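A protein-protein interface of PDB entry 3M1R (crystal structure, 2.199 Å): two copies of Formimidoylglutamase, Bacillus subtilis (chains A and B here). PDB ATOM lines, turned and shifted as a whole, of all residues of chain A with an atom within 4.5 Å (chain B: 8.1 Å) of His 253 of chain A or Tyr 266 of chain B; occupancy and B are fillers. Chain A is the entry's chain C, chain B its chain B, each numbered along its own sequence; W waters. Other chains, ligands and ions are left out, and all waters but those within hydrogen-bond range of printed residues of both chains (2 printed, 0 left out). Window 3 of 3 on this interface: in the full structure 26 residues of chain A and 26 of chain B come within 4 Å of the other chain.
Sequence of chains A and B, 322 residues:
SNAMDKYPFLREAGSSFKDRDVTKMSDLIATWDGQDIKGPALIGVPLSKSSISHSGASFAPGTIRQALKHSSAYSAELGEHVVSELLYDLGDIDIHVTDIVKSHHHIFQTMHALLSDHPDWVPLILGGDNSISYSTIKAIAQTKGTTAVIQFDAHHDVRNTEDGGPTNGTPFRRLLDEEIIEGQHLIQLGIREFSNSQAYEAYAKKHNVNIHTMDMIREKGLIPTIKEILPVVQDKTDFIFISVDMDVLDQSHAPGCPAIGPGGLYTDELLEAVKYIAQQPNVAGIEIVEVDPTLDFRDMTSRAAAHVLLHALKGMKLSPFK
OH of Tyr 266 of chain B is in hydrogen-bond range of OD2 of Asp 268 of chain A, 3.1 Å away.
The side-chain amide nitrogen (NE2) of Gln 251 of chain B is in hydrogen-bond range of the backbone carbonyl oxygen (O) of Met 300 of chain A (3.1 Å).
O of Ser 252 of chain A touches CB of Ser 252 of chain B, at 3.4 Å.
NE2 of His 253 of chain A touches OG of Ser 252 of chain B, 3.5 Å away.
His 253 of chain A touches Tyr 266 of chain B.
Thr 267 of chain A touches Pro 262 of chain B (CG2 to CB, 3.4 Å).
The side-chain hydroxyl (OG) of Ser 252 of chain B lies within hydrogen-bond range of the side-chain carboxylate (OD2) of Asp 250 of chain B, 2.7 Å away.
The side-chain carboxylate (OD2) of Asp 250 of chain A sits at hydrogen-bond distance from the side-chain hydroxyl (OG) of Ser 252 of chain A (2.7 Å).
The backbone NH of Tyr 266 of chain B is in hydrogen-bond range of the side-chain carboxylate of Glu 269 of chain B, at 2.6 Å.
The backbone NH (N) of Thr 267 of chain A is in hydrogen-bond range of a ring nitrogen (ND1) of His 253 of chain A (3.0 Å).
His 253 of chain A touches two residues of chain B.
Tyr 266 of chain B touches two residues of chain A.
Of the printed residues of chain A, Gln 251 of chain B touches Met 300.
Of the printed residues of chain B, Asp 268 of chain A touches Tyr 266 (3.1 Å).
Printed residues of chain B within 4 Å of Met 300 of chain A: Gln 251.
Printed residues of chain A within 4 Å of Ser 252 of chain B: Ser 252 (3.4 Å) and His 253 (3.5 Å).
Gln 251 of chain A touches none of the printed residues of chain B.
Leu 249 of chain B touches none of the printed residues of chain A.
The nearest printed residue of chain A that does not touch Tyr 266 of chain B is Tyr 266 of chain A (4.8 Å).
The nearest printed residue of chain A that does not touch Gln 251 of chain B is His 253 of chain A (4.7 Å).
Water W1 lies within hydrogen-bond range of the backbone carbonyl oxygen of His 253 of chain A (2.9 Å), the side-chain amide nitrogen of Gln 251 of chain B (3.0 Å) and the side-chain hydroxyl of Thr 267 of chain A (3.0 Å).
Water W2 lies within hydrogen-bond range of OD1 of Asp 250 of chain B (3.0 Å), OH of Tyr 266 of chain B (3.2 Å), N of Asp 268 of chain A (3.3 Å) and N of Gly 263 of chain B (3.3 Å).
Of the 22 printed residues of chain B, 4 touch a printed residue of chain A.
Hydrophobic or aromatic side chains of chain B that line the printed part of chain A: Pro 262 and Tyr 266.
Printed residues of chain A that touch a printed residue of chain B: Ser 252, His 253, Thr 267, Asp 268 and Met 300.
Among the printed residues, no Asp or Glu carboxylate lies within 4 Å of a Lys or Arg side-chain nitrogen of the other chain.
Ser 252 of chain A touches its own counterpart, Ser 252 of chain B.
His 253 of chain A touches Ser 252 of chain B, but with the chains exchanged Ser 252 of chain A does not touch His 253 of chain B (6.2 Å).
His 253 of chain A touches Tyr 266 of chain B, but with the chains exchanged Tyr 266 of chain A does not touch His 253 of chain B (7.7 Å).
Asp 268 of chain A touches Tyr 266 of chain B, but with the chains exchanged Tyr 266 of chain A does not touch Asp 268 of chain B (11.0 Å).
Positions printed for both chains: 250, 251, 252, 253, 254, 266, 267 and 268.
Of the 6 pairs that touch across the chains among the printed residues, 1 has its exchanged pair printed and touching as well.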
ATOM      1  N   ASP A 250      34.970 -12.092 -28.268  1.00  0.00           N
ATOM      2  CA  ASP A 250      34.182 -13.132 -27.621  1.00  0.00           C
ATOM      3  C   ASP A 250      32.981 -13.521 -28.462  1.00  0.00           C
ATOM      4  O   ASP A 250      32.369 -12.673 -29.113  1.00  0.00           O
ATOM      5  CB  ASP A 250      33.674 -12.657 -26.262  1.00  0.00           C
ATOM      6  CG  ASP A 250      33.197 -13.812 -25.384  1.00  0.00           C
ATOM      7  OD1 ASP A 250      34.057 -14.536 -24.849  1.00  0.00           O
ATOM      8  OD2 ASP A 250      31.969 -13.996 -25.234  1.00  0.00           O
ATOM      9  N   GLN A 251      32.616 -14.800 -28.435  1.00  0.00           N
ATOM     10  CA  GLN A 251      31.498 -15.238 -29.259  1.00  0.00           C
ATOM     11  C   GLN A 251      30.214 -14.456 -28.958  1.00  0.00           C
ATOM     12  O   GLN A 251      29.396 -14.243 -29.849  1.00  0.00           O
ATOM     13  CB  GLN A 251      31.257 -16.745 -29.151  1.00  0.00           C
ATOM     14  CG  GLN A 251      31.049 -17.288 -27.746  1.00  0.00           C
ATOM     15  CD  GLN A 251      30.790 -18.788 -27.793  1.00  0.00           C
ATOM     16  OE1 GLN A 251      30.846 -19.392 -28.865  1.00  0.00           O
ATOM     17  NE2 GLN A 251      30.483 -19.387 -26.648  1.00  0.00           N
ATOM     18  N   SER A 252      30.038 -14.031 -27.711  1.00  0.00           N
ATOM     19  CA  SER A 252      28.804 -13.337 -27.309  1.00  0.00           C
ATOM     20  C   SER A 252      28.765 -11.943 -27.932  1.00  0.00           C
ATOM     21  O   SER A 252      27.700 -11.361 -28.031  1.00  0.00           O
ATOM     22  CB  SER A 252      28.689 -13.219 -25.781  1.00  0.00           C
ATOM     23  OG  SER A 252      29.735 -12.403 -25.232  1.00  0.00           O
ATOM     24  N   HIS A 253      29.924 -11.431 -28.358  1.00  0.00           N
ATOM     25  CA  HIS A 253      30.000 -10.116 -29.001  1.00  0.00           C
ATOM     26  C   HIS A 253      30.162 -10.147 -30.516  1.00  0.00           C
ATOM     27  O   HIS A 253      29.950  -9.133 -31.186  1.00  0.00           O
ATOM     28  CB  HIS A 253      31.163  -9.311 -28.424  1.00  0.00           C
ATOM     29  CG  HIS A 253      30.859  -8.689 -27.106  1.00  0.00           C
ATOM     30  ND1 HIS A 253      31.190  -7.386 -26.811  1.00  0.00           N
ATOM     31  CD2 HIS A 253      30.258  -9.192 -26.001  1.00  0.00           C
ATOM     32  CE1 HIS A 253      30.803  -7.111 -25.576  1.00  0.00           C
ATOM     33  NE2 HIS A 253      30.241  -8.191 -25.063  1.00  0.00           N
ATOM     34  N   ALA A 254      30.583 -11.288 -31.046  1.00  0.00           N
ATOM     35  CA  ALA A 254      30.737 -11.465 -32.477  1.00  0.00           C
ATOM     36  C   ALA A 254      30.318 -12.874 -32.865  1.00  0.00           C
ATOM     37  O   ALA A 254      31.156 -13.685 -33.242  1.00  0.00           O
ATOM     38  CB  ALA A 254      32.200 -11.200 -32.908  1.00  0.00           C
ATOM     39  N   PRO A 255      29.010 -13.158 -32.806  1.00  0.00           N
ATOM     40  CA  PRO A 255      28.451 -14.474 -33.128  1.00  0.00           C
ATOM     41  C   PRO A 255      28.691 -14.849 -34.581  1.00  0.00           C
ATOM     42  O   PRO A 255      28.721 -16.031 -34.905  1.00  0.00           O
ATOM     43  CB  PRO A 255      26.939 -14.281 -32.950  1.00  0.00           C
ATOM     44  CG  PRO A 255      26.747 -12.931 -32.406  1.00  0.00           C
ATOM     45  CD  PRO A 255      27.974 -12.130 -32.634  1.00  0.00           C
ATOM     46  N   TYR A 266      36.048  -8.004 -25.688  1.00  0.00           N
ATOM     47  CA  TYR A 266      34.724  -7.387 -25.787  1.00  0.00           C
ATOM     48  C   TYR A 266      34.823  -6.200 -26.728  1.00  0.00           C
ATOM     49  O   TYR A 266      35.904  -5.609 -26.862  1.00  0.00           O
ATOM     50  CB  TYR A 266      34.182  -7.057 -24.390  1.00  0.00           C
ATOM     51  CG  TYR A 266      34.084  -8.359 -23.569  1.00  0.00           C
ATOM     52  CD1 TYR A 266      34.918  -8.599 -22.475  1.00  0.00           C
ATOM     53  CD2 TYR A 266      33.210  -9.382 -23.952  1.00  0.00           C
ATOM     54  CE1 TYR A 266      34.850  -9.798 -21.756  1.00  0.00           C
ATOM     55  CE2 TYR A 266      33.133 -10.589 -23.235  1.00  0.00           C
ATOM     56  CZ  TYR A 266      33.954 -10.790 -22.141  1.00  0.00           C
ATOM     57  OH  TYR A 266      33.884 -11.984 -21.436  1.00  0.00           O
ATOM     58  N   THR A 267      33.734  -5.890 -27.427  1.00  0.00           N
ATOM     59  CA  THR A 267      33.801  -4.940 -28.556  1.00  0.00           C
ATOM     60  C   THR A 267      34.265  -3.545 -28.132  1.00  0.00           C
ATOM     61  O   THR A 267      35.018  -2.903 -28.836  1.00  0.00           O
ATOM     62  CB  THR A 267      32.453  -4.830 -29.351  1.00  0.00           C
ATOM     63  OG1 THR A 267      32.095  -6.111 -29.850  1.00  0.00           O
ATOM     64  CG2 THR A 267      32.593  -3.911 -30.571  1.00  0.00           C
ATOM     65  N   ASP A 268      33.821  -3.082 -26.973  1.00  0.00           N
ATOM     66  CA  ASP A 268      34.214  -1.749 -26.529  1.00  0.00           C
ATOM     67  C   ASP A 268      35.735  -1.668 -26.284  1.00  0.00           C
ATOM     68  O   ASP A 268      36.367  -0.664 -26.629  1.00  0.00           O
ATOM     69  CB  ASP A 268      33.377  -1.282 -25.323  1.00  0.00           C
ATOM     70  CG  ASP A 268      33.307  -2.319 -24.201  1.00  0.00           C
ATOM     71  OD1 ASP A 268      34.134  -3.263 -24.177  1.00  0.00           O
ATOM     72  OD2 ASP A 268      32.415  -2.185 -23.329  1.00  0.00           O
ATOM     73  N   MET A 300      24.720  -8.069 -36.104  1.00  0.00           N
ATOM     74  CA  MET A 300      25.537  -7.645 -34.963  1.00  0.00           C
ATOM     75  C   MET A 300      27.009  -7.535 -35.295  1.00  0.00           C
ATOM     76  O   MET A 300      27.669  -6.560 -34.956  1.00  0.00           O
ATOM     77  CB  MET A 300      25.409  -8.635 -33.819  1.00  0.00           C
ATOM     78  CG  MET A 300      24.087  -8.552 -33.103  1.00  0.00           C
ATOM     79  SD  MET A 300      24.102  -9.821 -31.614  1.00  0.00           S
ATOM     80  CE  MET A 300      25.840  -9.399 -30.844  1.00  0.00           C
ATOM     81  N   MET B 214      28.139   7.372 -22.475  1.00  0.00           N
ATOM     82  CA  MET B 214      28.688   6.086 -22.055  1.00  0.00           C
ATOM     83  C   MET B 214      30.127   6.276 -21.591  1.00  0.00           C
ATOM     84  O   MET B 214      30.558   5.659 -20.623  1.00  0.00           O
ATOM     85  CB  MET B 214      28.652   5.085 -23.206  1.00  0.00           C
ATOM     86  CG  MET B 214      27.255   4.533 -23.513  1.00  0.00           C
ATOM     87  SD  MET B 214      26.559   3.533 -21.992  1.00  0.00           S
ATOM     88  CE  MET B 214      28.062   2.289 -21.782  1.00  0.00           C
ATOM     89  N   ARG B 218      31.344   5.159 -18.124  1.00  0.00           N
ATOM     90  CA  ARG B 218      32.376   4.151 -17.987  1.00  0.00           C
ATOM     91  C   ARG B 218      33.535   4.687 -17.146  1.00  0.00           C
ATOM     92  O   ARG B 218      34.231   3.919 -16.495  1.00  0.00           O
ATOM     93  CB  ARG B 218      32.871   3.700 -19.361  1.00  0.00           C
ATOM     94  CG  ARG B 218      31.897   2.780 -20.093  1.00  0.00           C
ATOM     95  CD  ARG B 218      32.124   1.344 -19.683  1.00  0.00           C
ATOM     96  NE  ARG B 218      31.050   0.469 -20.136  1.00  0.00           N
ATOM     97  CZ  ARG B 218      29.980   0.177 -19.404  1.00  0.00           C
ATOM     98  NH1 ARG B 218      29.847   0.692 -18.188  1.00  0.00           N
ATOM     99  NH2 ARG B 218      29.042  -0.621 -19.888  1.00  0.00           N
ATOM    100  N   LEU B 222      28.131   4.068 -13.335  1.00  0.00           N
ATOM    101  CA  LEU B 222      26.740   4.476 -13.488  1.00  0.00           C
ATOM    102  C   LEU B 222      26.116   4.978 -12.178  1.00  0.00           C
ATOM    103  O   LEU B 222      25.511   6.047 -12.145  1.00  0.00           O
ATOM    104  CB  LEU B 222      25.897   3.352 -14.116  1.00  0.00           C
ATOM    105  CG  LEU B 222      24.433   3.668 -14.438  1.00  0.00           C
ATOM    106  CD1 LEU B 222      24.324   4.992 -15.159  1.00  0.00           C
ATOM    107  CD2 LEU B 222      23.762   2.544 -15.254  1.00  0.00           C
ATOM    108  N   VAL B 248      19.471   1.266 -24.820  1.00  0.00           N
ATOM    109  CA  VAL B 248      20.556   1.778 -23.984  1.00  0.00           C
ATOM    110  C   VAL B 248      21.536   0.634 -23.715  1.00  0.00           C
ATOM    111  O   VAL B 248      22.710   0.853 -23.424  1.00  0.00           O
ATOM    112  CB  VAL B 248      20.022   2.329 -22.654  1.00  0.00           C
ATOM    113  CG1 VAL B 248      19.709   1.183 -21.704  1.00  0.00           C
ATOM    114  CG2 VAL B 248      21.025   3.275 -22.027  1.00  0.00           C
ATOM    115  N   LEU B 249      21.045  -0.599 -23.837  1.00  0.00           N
ATOM    116  CA  LEU B 249      21.851  -1.784 -23.530  1.00  0.00           C
ATOM    117  C   LEU B 249      22.682  -2.225 -24.714  1.00  0.00           C
ATOM    118  O   LEU B 249      22.238  -2.133 -25.855  1.00  0.00           O
ATOM    119  CB  LEU B 249      20.958  -2.954 -23.101  1.00  0.00           C
ATOM    120  CG  LEU B 249      20.292  -2.817 -21.735  1.00  0.00           C
ATOM    121  CD1 LEU B 249      19.167  -3.826 -21.573  1.00  0.00           C
ATOM    122  CD2 LEU B 249      21.332  -2.994 -20.658  1.00  0.00           C
ATOM    123  N   ASP B 250      23.887  -2.719 -24.433  1.00  0.00           N
ATOM    124  CA  ASP B 250      24.733  -3.293 -25.473  1.00  0.00           C
ATOM    125  C   ASP B 250      23.933  -4.305 -26.282  1.00  0.00           C
ATOM    126  O   ASP B 250      23.065  -4.976 -25.741  1.00  0.00           O
ATOM    127  CB  ASP B 250      25.954  -3.980 -24.862  1.00  0.00           C
ATOM    128  CG  ASP B 250      27.002  -4.338 -25.907  1.00  0.00           C
ATOM    129  OD1 ASP B 250      27.794  -3.437 -26.259  1.00  0.00           O
ATOM    130  OD2 ASP B 250      27.020  -5.504 -26.383  1.00  0.00           O
ATOM    131  N   GLN B 251      24.224  -4.406 -27.577  1.00  0.00           N
ATOM    132  CA  GLN B 251      23.523  -5.356 -28.434  1.00  0.00           C
ATOM    133  C   GLN B 251      23.653  -6.797 -27.927  1.00  0.00           C
ATOM    134  O   GLN B 251      22.688  -7.557 -27.974  1.00  0.00           O
ATOM    135  CB  GLN B 251      23.970  -5.228 -29.893  1.00  0.00           C
ATOM    136  CG  GLN B 251      25.448  -5.542 -30.177  1.00  0.00           C
ATOM    137  CD  GLN B 251      25.792  -5.257 -31.641  1.00  0.00           C
ATOM    138  OE1 GLN B 251      24.940  -4.790 -32.386  1.00  0.00           O
ATOM    139  NE2 GLN B 251      27.029  -5.542 -32.054  1.00  0.00           N
ATOM    140  N   SER B 252      24.829  -7.157 -27.416  1.00  0.00           N
ATOM    141  CA  SER B 252      25.033  -8.494 -26.861  1.00  0.00           C
ATOM    142  C   SER B 252      24.046  -8.788 -25.712  1.00  0.00           C
ATOM    143  O   SER B 252      23.705  -9.937 -25.460  1.00  0.00           O
ATOM    144  CB  SER B 252      26.484  -8.667 -26.362  1.00  0.00           C
ATOM    145  OG  SER B 252      26.718  -7.890 -25.179  1.00  0.00           O
ATOM    146  N   HIS B 253      23.607  -7.745 -25.018  1.00  0.00           N
ATOM    147  CA  HIS B 253      22.693  -7.909 -23.890  1.00  0.00           C
ATOM    148  C   HIS B 253      21.230  -7.666 -24.261  1.00  0.00           C
ATOM    149  O   HIS B 253      20.331  -8.124 -23.561  1.00  0.00           O
ATOM    150  CB  HIS B 253      23.093  -6.983 -22.732  1.00  0.00           C
ATOM    151  CG  HIS B 253      24.230  -7.503 -21.908  1.00  0.00           C
ATOM    152  ND1 HIS B 253      24.215  -7.514 -20.531  1.00  0.00           N
ATOM    153  CD2 HIS B 253      25.411  -8.059 -22.273  1.00  0.00           C
ATOM    154  CE1 HIS B 253      25.334  -8.050 -20.083  1.00  0.00           C
ATOM    155  NE2 HIS B 253      26.079  -8.381 -21.120  1.00  0.00           N
ATOM    156  N   ALA B 254      20.996  -6.957 -25.361  1.00  0.00           N
ATOM    157  CA  ALA B 254      19.631  -6.645 -25.777  1.00  0.00           C
ATOM    158  C   ALA B 254      19.531  -6.689 -27.292  1.00  0.00           C
ATOM    159  O   ALA B 254      19.396  -5.648 -27.943  1.00  0.00           O
ATOM    160  CB  ALA B 254      19.209  -5.258 -25.248  1.00  0.00           C
ATOM    161  N   PRO B 262      27.269  -1.876 -30.637  1.00  0.00           N
ATOM    162  CA  PRO B 262      28.204  -2.232 -29.564  1.00  0.00           C
ATOM    163  C   PRO B 262      28.471  -1.013 -28.708  1.00  0.00           C
ATOM    164  O   PRO B 262      28.216   0.114 -29.159  1.00  0.00           O
ATOM    165  CB  PRO B 262      29.456  -2.647 -30.329  1.00  0.00           C
ATOM    166  CG  PRO B 262      29.439  -1.736 -31.544  1.00  0.00           C
ATOM    167  CD  PRO B 262      27.963  -1.518 -31.889  1.00  0.00           C
ATOM    168  N   GLY B 263      28.946  -1.225 -27.484  1.00  0.00           N
ATOM    169  CA  GLY B 263      29.318  -0.113 -26.616  1.00  0.00           C
ATOM    170  C   GLY B 263      28.203   0.400 -25.714  1.00  0.00           C
ATOM    171  O   GLY B 263      28.218   1.567 -25.287  1.00  0.00           O
ATOM    172  N   GLY B 264      27.243  -0.466 -25.399  1.00  0.00           N
ATOM    173  CA  GLY B 264      26.147  -0.081 -24.531  1.00  0.00           C
ATOM    174  C   GLY B 264      26.323  -0.474 -23.074  1.00  0.00           C
ATOM    175  O   GLY B 264      27.374  -0.946 -22.681  1.00  0.00           O
ATOM    176  N   LEU B 265      25.284  -0.252 -22.271  1.00  0.00           N
ATOM    177  CA  LEU B 265      25.285  -0.621 -20.861  1.00  0.00           C
ATOM    178  C   LEU B 265      25.109  -2.125 -20.761  1.00  0.00           C
ATOM    179  O   LEU B 265      24.631  -2.751 -21.698  1.00  0.00           O
ATOM    180  CB  LEU B 265      24.113   0.064 -20.135  1.00  0.00           C
ATOM    181  CG  LEU B 265      24.215   1.522 -19.691  1.00  0.00           C
ATOM    182  CD1 LEU B 265      22.927   1.937 -18.973  1.00  0.00           C
ATOM    183  CD2 LEU B 265      25.445   1.717 -18.795  1.00  0.00           C
ATOM    184  N   TYR B 266      25.461  -2.711 -19.631  1.00  0.00           N
ATOM    185  CA  TYR B 266      25.156  -4.129 -19.425  1.00  0.00           C
ATOM    186  C   TYR B 266      23.969  -4.246 -18.470  1.00  0.00           C
ATOM    187  O   TYR B 266      23.720  -3.346 -17.675  1.00  0.00           O
ATOM    188  CB  TYR B 266      26.394  -4.908 -18.991  1.00  0.00           C
ATOM    189  CG  TYR B 266      27.479  -4.819 -20.049  1.00  0.00           C
ATOM    190  CD1 TYR B 266      28.540  -3.933 -19.913  1.00  0.00           C
ATOM    191  CD2 TYR B 266      27.409  -5.581 -21.211  1.00  0.00           C
ATOM    192  CE1 TYR B 266      29.514  -3.829 -20.888  1.00  0.00           C
ATOM    193  CE2 TYR B 266      28.381  -5.485 -22.199  1.00  0.00           C
ATOM    194  CZ  TYR B 266      29.433  -4.608 -22.036  1.00  0.00           C
ATOM    195  OH  TYR B 266      30.411  -4.507 -23.010  1.00  0.00           O
ATOM    196  N   THR B 267      23.188  -5.309 -18.603  1.00  0.00           N
ATOM    197  CA  THR B 267      21.911  -5.382 -17.893  1.00  0.00           C
ATOM    198  C   THR B 267      22.129  -5.273 -16.375  1.00  0.00           C
ATOM    199  O   THR B 267      21.356  -4.625 -15.681  1.00  0.00           O
ATOM    200  CB  THR B 267      21.112  -6.651 -18.281  1.00  0.00           C
ATOM    201  OG1 THR B 267      21.071  -6.760 -19.704  1.00  0.00           O
ATOM    202  CG2 THR B 267      19.676  -6.566 -17.782  1.00  0.00           C
ATOM    203  N   ASP B 268      23.186  -5.926 -15.889  1.00  0.00           N
ATOM    204  CA  ASP B 268      23.699  -5.790 -14.518  1.00  0.00           C
ATOM    205  C   ASP B 268      23.601  -4.357 -14.014  1.00  0.00           C
ATOM    206  O   ASP B 268      22.945  -4.082 -13.014  1.00  0.00           O
ATOM    207  CB  ASP B 268      25.201  -6.159 -14.451  1.00  0.00           C
ATOM    208  CG  ASP B 268      25.520  -7.558 -14.977  1.00  0.00           C
ATOM    209  OD1 ASP B 268      26.342  -8.248 -14.332  1.00  0.00           O
ATOM    210  OD2 ASP B 268      24.987  -7.967 -16.035  1.00  0.00           O
ATOM    211  N   GLU B 269      24.309  -3.454 -14.690  1.00  0.00           N
ATOM    212  CA  GLU B 269      24.386  -2.061 -14.262  1.00  0.00           C
ATOM    213  C   GLU B 269      23.011  -1.434 -14.280  1.00  0.00           C
ATOM    214  O   GLU B 269      22.647  -0.722 -13.342  1.00  0.00           O
ATOM    215  CB  GLU B 269      25.317  -1.228 -15.153  1.00  0.00           C
ATOM    216  CG  GLU B 269      26.127  -2.014 -16.143  1.00  0.00           C
ATOM    217  CD  GLU B 269      27.035  -1.133 -16.988  1.00  0.00           C
ATOM    218  OE1 GLU B 269      27.156  -1.417 -18.193  1.00  0.00           O
ATOM    219  OE2 GLU B 269      27.634  -0.168 -16.458  1.00  0.00           O
ATOM    220  N   LEU B 270      22.250  -1.706 -15.344  1.00  0.00           N
ATOM    221  CA  LEU B 270      20.926  -1.099 -15.511  1.00  0.00           C
ATOM    222  C   LEU B 270      20.002  -1.507 -14.396  1.00  0.00           C
ATOM    223  O   LEU B 270      19.283  -0.684 -13.849  1.00  0.00           O
ATOM    224  CB  LEU B 270      20.294  -1.473 -16.848  1.00  0.00           C
ATOM    225  CG  LEU B 270      18.901  -0.922 -17.109  1.00  0.00           C
ATOM    226  CD1 LEU B 270      18.914   0.589 -17.047  1.00  0.00           C
ATOM    227  CD2 LEU B 270      18.386  -1.414 -18.483  1.00  0.00           C
ATOM    228  N   LEU B 271      20.009  -2.789 -14.071  1.00  0.00           N
ATOM    229  CA  LEU B 271      19.141  -3.294 -13.020  1.00  0.00           C
ATOM    230  C   LEU B 271      19.422  -2.546 -11.719  1.00  0.00           C
ATOM    231  O   LEU B 271      18.510  -2.027 -11.068  1.00  0.00           O
ATOM    232  CB  LEU B 271      19.358  -4.789 -12.849  1.00  0.00           C
ATOM    233  CG  LEU B 271      18.305  -5.686 -13.509  1.00  0.00           C
ATOM    234  CD1 LEU B 271      17.509  -4.964 -14.584  1.00  0.00           C
ATOM    235  CD2 LEU B 271      18.940  -6.923 -14.066  1.00  0.00           C
ATOM    236  N   GLU B 272      20.699  -2.471 -11.368  1.00  0.00           N
ATOM    237  CA  GLU B 272      21.137  -1.841 -10.117  1.00  0.00           C
ATOM    238  C   GLU B 272      20.777  -0.356 -10.120  1.00  0.00           C
ATOM    239  O   GLU B 272      20.332   0.177  -9.118  1.00  0.00           O
ATOM    240  CB  GLU B 272      22.654  -2.044  -9.938  1.00  0.00           C
ATOM    241  CG  GLU B 272      23.260  -1.587  -8.631  1.00  0.00           C
ATOM    242  CD  GLU B 272      24.787  -1.677  -8.656  1.00  0.00           C
ATOM    243  OE1 GLU B 272      25.414  -1.661  -7.571  1.00  0.00           O
ATOM    244  OE2 GLU B 272      25.364  -1.770  -9.766  1.00  0.00           O
ATOM    245  N   ALA B 273      20.959   0.305 -11.258  1.00  0.00           N
ATOM    246  CA  ALA B 273      20.576   1.709 -11.388  1.00  0.00           C
ATOM    247  C   ALA B 273      19.064   1.948 -11.216  1.00  0.00           C
ATOM    248  O   ALA B 273      18.657   2.859 -10.518  1.00  0.00           O
ATOM    249  CB  ALA B 273      21.068   2.273 -12.712  1.00  0.00           C
HETATM  250  O   HOH W   1      29.170  -6.540 -30.284  1.00  0.00           O
HETATM  251  O   HOH W   2      30.754  -3.614 -26.034  1.00  0.00           O
